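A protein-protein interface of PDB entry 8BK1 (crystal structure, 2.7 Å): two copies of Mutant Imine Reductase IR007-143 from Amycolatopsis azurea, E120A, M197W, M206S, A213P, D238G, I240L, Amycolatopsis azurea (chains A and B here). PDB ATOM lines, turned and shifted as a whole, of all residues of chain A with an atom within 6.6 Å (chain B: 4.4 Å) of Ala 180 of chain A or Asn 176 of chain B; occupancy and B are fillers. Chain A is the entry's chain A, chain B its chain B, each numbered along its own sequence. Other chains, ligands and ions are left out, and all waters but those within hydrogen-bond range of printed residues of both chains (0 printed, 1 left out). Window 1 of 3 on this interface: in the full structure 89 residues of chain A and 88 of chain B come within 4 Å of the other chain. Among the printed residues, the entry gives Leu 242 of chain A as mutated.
The side-chain amide nitrogen (ND2) of Asn 176 of chain A lies close to the side-chain amide oxygen (OD1) of Asn 176 of chain B, 2.3 Å away. A ring nitrogen (ND1) of His 183 of chain A is in hydrogen-bond range of the side-chain carboxylate of Asp 172 of chain B, 2.4 Å away. OD2 of Asp 172 of chain B is in hydrogen-bond range of N of Ala 184 of chain A (3.3 Å).
The backbone carbonyl oxygen (O) of Asp 172 of chain B lies close to the side-chain amide nitrogen (ND2) of Asn 176 of chain B, 3.4 Å away. The backbone carbonyl oxygen (O) of Ile 173 of chain B is in hydrogen-bond range of the side-chain hydroxyl (OG) of Ser 177 of chain B (2.9 Å).
CB of Ala 180 of chain B touches CB of Asn 176 of chain A (3.7 Å). CD2 of Leu 255 of chain B touches OD1 of Asn 176 of chain A, 3.7 Å away. Asn 176 of chain B touches Ala 180 of chain A (CB to CB, 3.7 Å). Phe 206 of chain A touches Ile 173 of chain B (CZ to CG2, 3.4 Å). Leu 242 of chain A touches Asp 172 of chain B. CD2 of Leu 255 of chain A touches ND2 of Asn 176 of chain B (3.6 Å). CB of Leu 175 of chain B touches CG1 of Val 259 of chain A, at 3.9 Å. CG2 of Val 259 of chain A touches ND2 of Asn 176 of chain B (3.6 Å). Val 259 of chain A touches Leu 255 of chain B (CG2 to CD1, 3.9 Å).
Ala 180 of chain A touches just one residue of chain B: Asn 176. Asn 176 of chain B touches just these residues of chain A: Asn 176, Ala 180, Leu 255 and Val 259. Of the printed residues of chain B, His 183 of chain A touches Asp 172 (2.4 Å). Printed residues of chain B within 4 Å of Leu 242 of chain A: Asp 172. Printed residues of chain A within 4 Å of Ala 180 of chain B: Asn 176 (3.7 Å). Ser 179 of chain A touches none of the printed residues of chain B. Ala 186 of chain A touches none of the printed residues of chain B. The nearest printed residue of chain A that does not touch Ile 173 of chain B is Ala 184 of chain A (4.04 Å).
Of the 10 printed residues of chain B, 6 touch a printed residue of chain A. Hydrophobic or aromatic side chains of chain A that line the printed part of chain B: Ala 180, His 183, Ala 184, Phe 206, Leu 242, Leu 255 and Val 259. Among the printed residues, 12 pairs touch across the chains. Among the printed residues, no Asp or Glu carboxylate lies within 4 Å of a Lys or Arg side-chain nitrogen of the other chain.
Asn 176 of chain B touches its own counterpart, Asn 176 of chain A. Asn 176 of chain A touches Ala 180 of chain B, and with the chains exchanged Ala 180 of chain A touches Asn 176 of chain B. Asn 176 of chain A touches Leu 255 of chain B, and with the chains exchanged Leu 255 of chain A touches Asn 176 of chain B.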
ATOM      1  N   LEU A 175      -8.180 -27.138 -13.513  1.00  0.00           N
ATOM      2  CA  LEU A 175      -7.132 -27.182 -14.571  1.00  0.00           C
ATOM      3  C   LEU A 175      -7.324 -26.023 -15.562  1.00  0.00           C
ATOM      4  O   LEU A 175      -6.319 -25.467 -16.021  1.00  0.00           O
ATOM      5  CB  LEU A 175      -7.134 -28.533 -15.290  1.00  0.00           C
ATOM      6  CG  LEU A 175      -6.799 -29.724 -14.409  1.00  0.00           C
ATOM      7  CD1 LEU A 175      -6.732 -31.002 -15.228  1.00  0.00           C
ATOM      8  CD2 LEU A 175      -5.500 -29.511 -13.702  1.00  0.00           C
ATOM      9  N   ASN A 176      -8.564 -25.668 -15.850  1.00  0.00           N
ATOM     10  CA  ASN A 176      -8.885 -24.545 -16.748  1.00  0.00           C
ATOM     11  C   ASN A 176      -8.324 -23.256 -16.174  1.00  0.00           C
ATOM     12  O   ASN A 176      -7.714 -22.466 -16.916  1.00  0.00           O
ATOM     13  CB  ASN A 176     -10.386 -24.325 -16.924  1.00  0.00           C
ATOM     14  CG  ASN A 176     -10.744 -24.626 -18.343  1.00  0.00           C
ATOM     15  OD1 ASN A 176     -11.008 -25.784 -18.638  1.00  0.00           O
ATOM     16  ND2 ASN A 176     -10.629 -23.625 -19.207  1.00  0.00           N
ATOM     17  N   SER A 177      -8.596 -23.035 -14.902  1.00  0.00           N
ATOM     18  CA  SER A 177      -8.169 -21.818 -14.207  1.00  0.00           C
ATOM     19  C   SER A 177      -6.640 -21.709 -14.307  1.00  0.00           C
ATOM     20  O   SER A 177      -6.163 -20.622 -14.716  1.00  0.00           O
ATOM     21  CB  SER A 177      -8.706 -21.811 -12.814  1.00  0.00           C
ATOM     22  OG  SER A 177     -10.114 -21.667 -12.842  1.00  0.00           O
ATOM     23  N   LEU A 178      -5.900 -22.792 -14.049  1.00  0.00           N
ATOM     24  CA  LEU A 178      -4.411 -22.787 -14.153  1.00  0.00           C
ATOM     25  C   LEU A 178      -4.016 -22.419 -15.582  1.00  0.00           C
ATOM     26  O   LEU A 178      -3.207 -21.483 -15.769  1.00  0.00           O
ATOM     27  CB  LEU A 178      -3.836 -24.155 -13.783  1.00  0.00           C
ATOM     28  CG  LEU A 178      -4.215 -24.720 -12.416  1.00  0.00           C
ATOM     29  CD1 LEU A 178      -3.375 -25.924 -12.060  1.00  0.00           C
ATOM     30  CD2 LEU A 178      -4.106 -23.678 -11.345  1.00  0.00           C
ATOM     31  N   SER A 179      -4.565 -23.124 -16.558  1.00  0.00           N
ATOM     32  CA  SER A 179      -4.156 -22.943 -17.960  1.00  0.00           C
ATOM     33  C   SER A 179      -4.522 -21.524 -18.370  1.00  0.00           C
ATOM     34  O   SER A 179      -3.761 -20.893 -19.117  1.00  0.00           O
ATOM     35  CB  SER A 179      -4.718 -23.991 -18.889  1.00  0.00           C
ATOM     36  OG  SER A 179      -4.024 -25.222 -18.743  1.00  0.00           O
ATOM     37  N   ALA A 180      -5.619 -20.988 -17.870  1.00  0.00           N
ATOM     38  CA  ALA A 180      -6.067 -19.641 -18.299  1.00  0.00           C
ATOM     39  C   ALA A 180      -5.159 -18.590 -17.651  1.00  0.00           C
ATOM     40  O   ALA A 180      -4.728 -17.632 -18.331  1.00  0.00           O
ATOM     41  CB  ALA A 180      -7.499 -19.430 -17.960  1.00  0.00           C
ATOM     42  N   PHE A 181      -4.860 -18.769 -16.378  1.00  0.00           N
ATOM     43  CA  PHE A 181      -3.904 -17.902 -15.654  1.00  0.00           C
ATOM     44  C   PHE A 181      -2.569 -17.884 -16.421  1.00  0.00           C
ATOM     45  O   PHE A 181      -2.078 -16.768 -16.731  1.00  0.00           O
ATOM     46  CB  PHE A 181      -3.721 -18.394 -14.218  1.00  0.00           C
ATOM     47  CG  PHE A 181      -2.687 -17.594 -13.495  1.00  0.00           C
ATOM     48  CD1 PHE A 181      -2.885 -16.247 -13.307  1.00  0.00           C
ATOM     49  CD2 PHE A 181      -1.515 -18.161 -13.066  1.00  0.00           C
ATOM     50  CE1 PHE A 181      -1.970 -15.480 -12.615  1.00  0.00           C
ATOM     51  CE2 PHE A 181      -0.599 -17.403 -12.353  1.00  0.00           C
ATOM     52  CZ  PHE A 181      -0.810 -16.058 -12.167  1.00  0.00           C
ATOM     53  N   MET A 182      -2.038 -19.068 -16.784  1.00  0.00           N
ATOM     54  CA  MET A 182      -0.734 -19.177 -17.480  1.00  0.00           C
ATOM     55  C   MET A 182      -0.866 -18.535 -18.865  1.00  0.00           C
ATOM     56  O   MET A 182       0.046 -17.821 -19.263  1.00  0.00           O
ATOM     57  CB  MET A 182      -0.245 -20.628 -17.562  1.00  0.00           C
ATOM     58  CG  MET A 182       0.271 -21.104 -16.209  1.00  0.00           C
ATOM     59  SD  MET A 182       0.863 -22.789 -16.121  1.00  0.00           S
ATOM     60  CE  MET A 182      -0.606 -23.726 -16.550  1.00  0.00           C
ATOM     61  N   HIS A 183      -1.999 -18.710 -19.537  1.00  0.00           N
ATOM     62  CA  HIS A 183      -2.223 -18.148 -20.894  1.00  0.00           C
ATOM     63  C   HIS A 183      -2.231 -16.620 -20.827  1.00  0.00           C
ATOM     64  O   HIS A 183      -1.566 -15.972 -21.670  1.00  0.00           O
ATOM     65  CB  HIS A 183      -3.518 -18.686 -21.519  1.00  0.00           C
ATOM     66  CG  HIS A 183      -3.591 -18.419 -22.988  1.00  0.00           C
ATOM     67  ND1 HIS A 183      -4.065 -17.222 -23.474  1.00  0.00           N
ATOM     68  CD2 HIS A 183      -3.177 -19.151 -24.054  1.00  0.00           C
ATOM     69  CE1 HIS A 183      -4.003 -17.241 -24.784  1.00  0.00           C
ATOM     70  NE2 HIS A 183      -3.445 -18.414 -25.173  1.00  0.00           N
ATOM     71  N   ALA A 184      -2.973 -16.059 -19.879  1.00  0.00           N
ATOM     72  CA  ALA A 184      -3.065 -14.604 -19.709  1.00  0.00           C
ATOM     73  C   ALA A 184      -1.662 -14.094 -19.364  1.00  0.00           C
ATOM     74  O   ALA A 184      -1.216 -13.134 -20.007  1.00  0.00           O
ATOM     75  CB  ALA A 184      -4.072 -14.267 -18.652  1.00  0.00           C
ATOM     76  N   SER A 185      -0.990 -14.750 -18.420  1.00  0.00           N
ATOM     77  CA  SER A 185       0.407 -14.434 -18.001  1.00  0.00           C
ATOM     78  C   SER A 185       1.299 -14.421 -19.247  1.00  0.00           C
ATOM     79  O   SER A 185       2.010 -13.425 -19.461  1.00  0.00           O
ATOM     80  CB  SER A 185       0.900 -15.411 -16.971  1.00  0.00           C
ATOM     81  OG  SER A 185       0.154 -15.291 -15.743  1.00  0.00           O
ATOM     82  N   ALA A 186       1.175 -15.437 -20.100  1.00  0.00           N
ATOM     83  CA  ALA A 186       1.975 -15.575 -21.330  1.00  0.00           C
ATOM     84  C   ALA A 186       1.714 -14.372 -22.255  1.00  0.00           C
ATOM     85  O   ALA A 186       2.663 -13.911 -22.920  1.00  0.00           O
ATOM     86  CB  ALA A 186       1.688 -16.890 -22.017  1.00  0.00           C
ATOM     87  N   PHE A 206     -10.349 -13.588 -10.458  1.00  0.00           N
ATOM     88  CA  PHE A 206     -10.740 -14.888  -9.874  1.00  0.00           C
ATOM     89  C   PHE A 206     -11.598 -14.685  -8.612  1.00  0.00           C
ATOM     90  O   PHE A 206     -12.511 -15.463  -8.372  1.00  0.00           O
ATOM     91  CB  PHE A 206      -9.514 -15.750  -9.573  1.00  0.00           C
ATOM     92  CG  PHE A 206      -8.941 -16.455 -10.773  1.00  0.00           C
ATOM     93  CD1 PHE A 206      -9.614 -17.523 -11.371  1.00  0.00           C
ATOM     94  CD2 PHE A 206      -7.732 -16.032 -11.319  1.00  0.00           C
ATOM     95  CE1 PHE A 206      -9.091 -18.154 -12.490  1.00  0.00           C
ATOM     96  CE2 PHE A 206      -7.201 -16.675 -12.430  1.00  0.00           C
ATOM     97  CZ  PHE A 206      -7.887 -17.725 -13.021  1.00  0.00           C
ATOM     98  N   LEU A 242      -9.146 -12.233 -28.647  1.00  0.00           N
ATOM     99  CA  LEU A 242      -8.184 -12.971 -27.809  1.00  0.00           C
ATOM    100  C   LEU A 242      -7.401 -13.922 -28.718  1.00  0.00           C
ATOM    101  O   LEU A 242      -6.148 -13.979 -28.619  1.00  0.00           O
ATOM    102  CB  LEU A 242      -8.917 -13.720 -26.697  1.00  0.00           C
ATOM    103  CG  LEU A 242      -7.979 -14.466 -25.757  1.00  0.00           C
ATOM    104  CD1 LEU A 242      -6.921 -13.512 -25.234  1.00  0.00           C
ATOM    105  CD2 LEU A 242      -8.726 -15.138 -24.602  1.00  0.00           C
ATOM    106  N   LEU A 255      -6.179 -23.079 -26.373  1.00  0.00           N
ATOM    107  CA  LEU A 255      -7.134 -22.689 -25.313  1.00  0.00           C
ATOM    108  C   LEU A 255      -8.073 -21.610 -25.844  1.00  0.00           C
ATOM    109  O   LEU A 255      -9.284 -21.743 -25.790  1.00  0.00           O
ATOM    110  CB  LEU A 255      -6.368 -22.221 -24.071  1.00  0.00           C
ATOM    111  CG  LEU A 255      -7.219 -22.207 -22.808  1.00  0.00           C
ATOM    112  CD1 LEU A 255      -7.587 -23.623 -22.427  1.00  0.00           C
ATOM    113  CD2 LEU A 255      -6.548 -21.486 -21.660  1.00  0.00           C
ATOM    114  N   PRO A 256      -7.590 -20.481 -26.387  1.00  0.00           N
ATOM    115  CA  PRO A 256      -8.522 -19.445 -26.826  1.00  0.00           C
ATOM    116  C   PRO A 256      -9.362 -19.913 -28.021  1.00  0.00           C
ATOM    117  O   PRO A 256     -10.492 -19.516 -28.088  1.00  0.00           O
ATOM    118  CB  PRO A 256      -7.634 -18.235 -27.086  1.00  0.00           C
ATOM    119  CG  PRO A 256      -6.252 -18.834 -27.312  1.00  0.00           C
ATOM    120  CD  PRO A 256      -6.184 -20.099 -26.502  1.00  0.00           C
ATOM    121  N   VAL A 259     -12.347 -21.877 -26.527  1.00  0.00           N
ATOM    122  CA  VAL A 259     -13.355 -20.942 -25.958  1.00  0.00           C
ATOM    123  C   VAL A 259     -14.106 -20.252 -27.110  1.00  0.00           C
ATOM    124  O   VAL A 259     -15.335 -20.184 -27.043  1.00  0.00           O
ATOM    125  CB  VAL A 259     -12.680 -19.948 -25.010  1.00  0.00           C
ATOM    126  CG1 VAL A 259     -13.641 -18.844 -24.608  1.00  0.00           C
ATOM    127  CG2 VAL A 259     -12.131 -20.664 -23.778  1.00  0.00           C
ATOM    128  N   ASP B 172      -9.308 -13.306 -21.029  1.00  0.00           N
ATOM    129  CA  ASP B 172      -8.767 -14.678 -21.159  1.00  0.00           C
ATOM    130  C   ASP B 172      -9.223 -15.444 -19.913  1.00  0.00           C
ATOM    131  O   ASP B 172      -9.880 -16.475 -20.048  1.00  0.00           O
ATOM    132  CB  ASP B 172      -7.268 -14.557 -21.404  1.00  0.00           C
ATOM    133  CG  ASP B 172      -6.560 -15.811 -21.806  1.00  0.00           C
ATOM    134  OD1 ASP B 172      -7.203 -16.870 -21.772  1.00  0.00           O
ATOM    135  OD2 ASP B 172      -5.345 -15.691 -22.125  1.00  0.00           O
ATOM    136  N   ILE B 173      -8.958 -14.917 -18.728  1.00  0.00           N
ATOM    137  CA  ILE B 173      -9.336 -15.610 -17.466  1.00  0.00           C
ATOM    138  C   ILE B 173     -10.866 -15.668 -17.377  1.00  0.00           C
ATOM    139  O   ILE B 173     -11.433 -16.732 -16.993  1.00  0.00           O
ATOM    140  CB  ILE B 173      -8.703 -14.895 -16.264  1.00  0.00           C
ATOM    141  CG1 ILE B 173      -7.190 -15.130 -16.235  1.00  0.00           C
ATOM    142  CG2 ILE B 173      -9.363 -15.331 -14.969  1.00  0.00           C
ATOM    143  CD1 ILE B 173      -6.430 -14.187 -15.332  1.00  0.00           C
ATOM    144  N   PHE B 174     -11.514 -14.560 -17.712  1.00  0.00           N
ATOM    145  CA  PHE B 174     -12.967 -14.400 -17.522  1.00  0.00           C
ATOM    146  C   PHE B 174     -13.733 -15.399 -18.416  1.00  0.00           C
ATOM    147  O   PHE B 174     -14.509 -16.209 -17.861  1.00  0.00           O
ATOM    148  CB  PHE B 174     -13.380 -12.963 -17.773  1.00  0.00           C
ATOM    149  CG  PHE B 174     -14.824 -12.708 -17.436  1.00  0.00           C
ATOM    150  CD1 PHE B 174     -15.240 -12.752 -16.122  1.00  0.00           C
ATOM    151  CD2 PHE B 174     -15.748 -12.384 -18.420  1.00  0.00           C
ATOM    152  CE1 PHE B 174     -16.555 -12.486 -15.791  1.00  0.00           C
ATOM    153  CE2 PHE B 174     -17.066 -12.130 -18.090  1.00  0.00           C
ATOM    154  CZ  PHE B 174     -17.467 -12.204 -16.780  1.00  0.00           C
ATOM    155  N   LEU B 175     -13.508 -15.395 -19.734  1.00  0.00           N
ATOM    156  CA  LEU B 175     -14.304 -16.243 -20.654  1.00  0.00           C
ATOM    157  C   LEU B 175     -14.003 -17.721 -20.372  1.00  0.00           C
ATOM    158  O   LEU B 175     -14.922 -18.546 -20.473  1.00  0.00           O
ATOM    159  CB  LEU B 175     -13.994 -15.908 -22.118  1.00  0.00           C
ATOM    160  CG  LEU B 175     -14.280 -14.492 -22.577  1.00  0.00           C
ATOM    161  CD1 LEU B 175     -14.005 -14.368 -24.062  1.00  0.00           C
ATOM    162  CD2 LEU B 175     -15.683 -14.078 -22.228  1.00  0.00           C
ATOM    163  N   ASN B 176     -12.768 -18.037 -20.000  1.00  0.00           N
ATOM    164  CA  ASN B 176     -12.378 -19.408 -19.625  1.00  0.00           C
ATOM    165  C   ASN B 176     -13.190 -19.876 -18.434  1.00  0.00           C
ATOM    166  O   ASN B 176     -13.713 -21.010 -18.475  1.00  0.00           O
ATOM    167  CB  ASN B 176     -10.917 -19.522 -19.251  1.00  0.00           C
ATOM    168  CG  ASN B 176     -10.221 -20.344 -20.300  1.00  0.00           C
ATOM    169  OD1 ASN B 176     -10.264 -21.571 -20.199  1.00  0.00           O
ATOM    170  ND2 ASN B 176      -9.659 -19.666 -21.305  1.00  0.00           N
ATOM    171  N   SER B 177     -13.247 -19.038 -17.412  1.00  0.00           N
ATOM    172  CA  SER B 177     -13.970 -19.360 -16.168  1.00  0.00           C
ATOM    173  C   SER B 177     -15.435 -19.667 -16.517  1.00  0.00           C
ATOM    174  O   SER B 177     -15.926 -20.721 -16.052  1.00  0.00           O
ATOM    175  CB  SER B 177     -13.810 -18.255 -15.166  1.00  0.00           C
ATOM    176  OG  SER B 177     -12.467 -18.193 -14.731  1.00  0.00           O
ATOM    177  N   LEU B 178     -16.087 -18.840 -17.357  1.00  0.00           N
ATOM    178  CA  LEU B 178     -17.502 -19.065 -17.761  1.00  0.00           C
ATOM    179  C   LEU B 178     -17.599 -20.428 -18.452  1.00  0.00           C
ATOM    180  O   LEU B 178     -18.458 -21.280 -18.044  1.00  0.00           O
ATOM    181  CB  LEU B 178     -17.984 -17.950 -18.695  1.00  0.00           C
ATOM    182  CG  LEU B 178     -17.881 -16.516 -18.155  1.00  0.00           C
ATOM    183  CD1 LEU B 178     -18.666 -15.530 -18.979  1.00  0.00           C
ATOM    184  CD2 LEU B 178     -18.341 -16.400 -16.736  1.00  0.00           C
ATOM    185  N   SER B 179     -16.758 -20.639 -19.466  1.00  0.00           N
ATOM    186  CA  SER B 179     -16.858 -21.862 -20.285  1.00  0.00           C
ATOM    187  C   SER B 179     -16.569 -23.062 -19.381  1.00  0.00           C
ATOM    188  O   SER B 179     -17.205 -24.106 -19.540  1.00  0.00           O
ATOM    189  CB  SER B 179     -16.012 -21.810 -21.517  1.00  0.00           C
ATOM    190  OG  SER B 179     -16.592 -20.950 -22.502  1.00  0.00           O
ATOM    191  N   ALA B 180     -15.675 -22.914 -18.416  1.00  0.00           N
ATOM    192  CA  ALA B 180     -15.274 -24.046 -17.554  1.00  0.00           C
ATOM    193  C   ALA B 180     -16.435 -24.357 -16.602  1.00  0.00           C
ATOM    194  O   ALA B 180     -16.784 -25.566 -16.407  1.00  0.00           O
ATOM    195  CB  ALA B 180     -14.001 -23.738 -16.811  1.00  0.00           C
ATOM    196  N   LEU B 255     -12.814 -27.802 -25.110  1.00  0.00           N
ATOM    197  CA  LEU B 255     -12.170 -27.160 -23.939  1.00  0.00           C
ATOM    198  C   LEU B 255     -11.248 -28.171 -23.258  1.00  0.00           C
ATOM    199  O   LEU B 255     -10.072 -27.913 -23.055  1.00  0.00           O
ATOM    200  CB  LEU B 255     -13.245 -26.626 -22.985  1.00  0.00           C
ATOM    201  CG  LEU B 255     -12.739 -25.649 -21.924  1.00  0.00           C
ATOM    202  CD1 LEU B 255     -12.234 -24.378 -22.576  1.00  0.00           C
ATOM    203  CD2 LEU B 255     -13.828 -25.313 -20.919  1.00  0.00           C
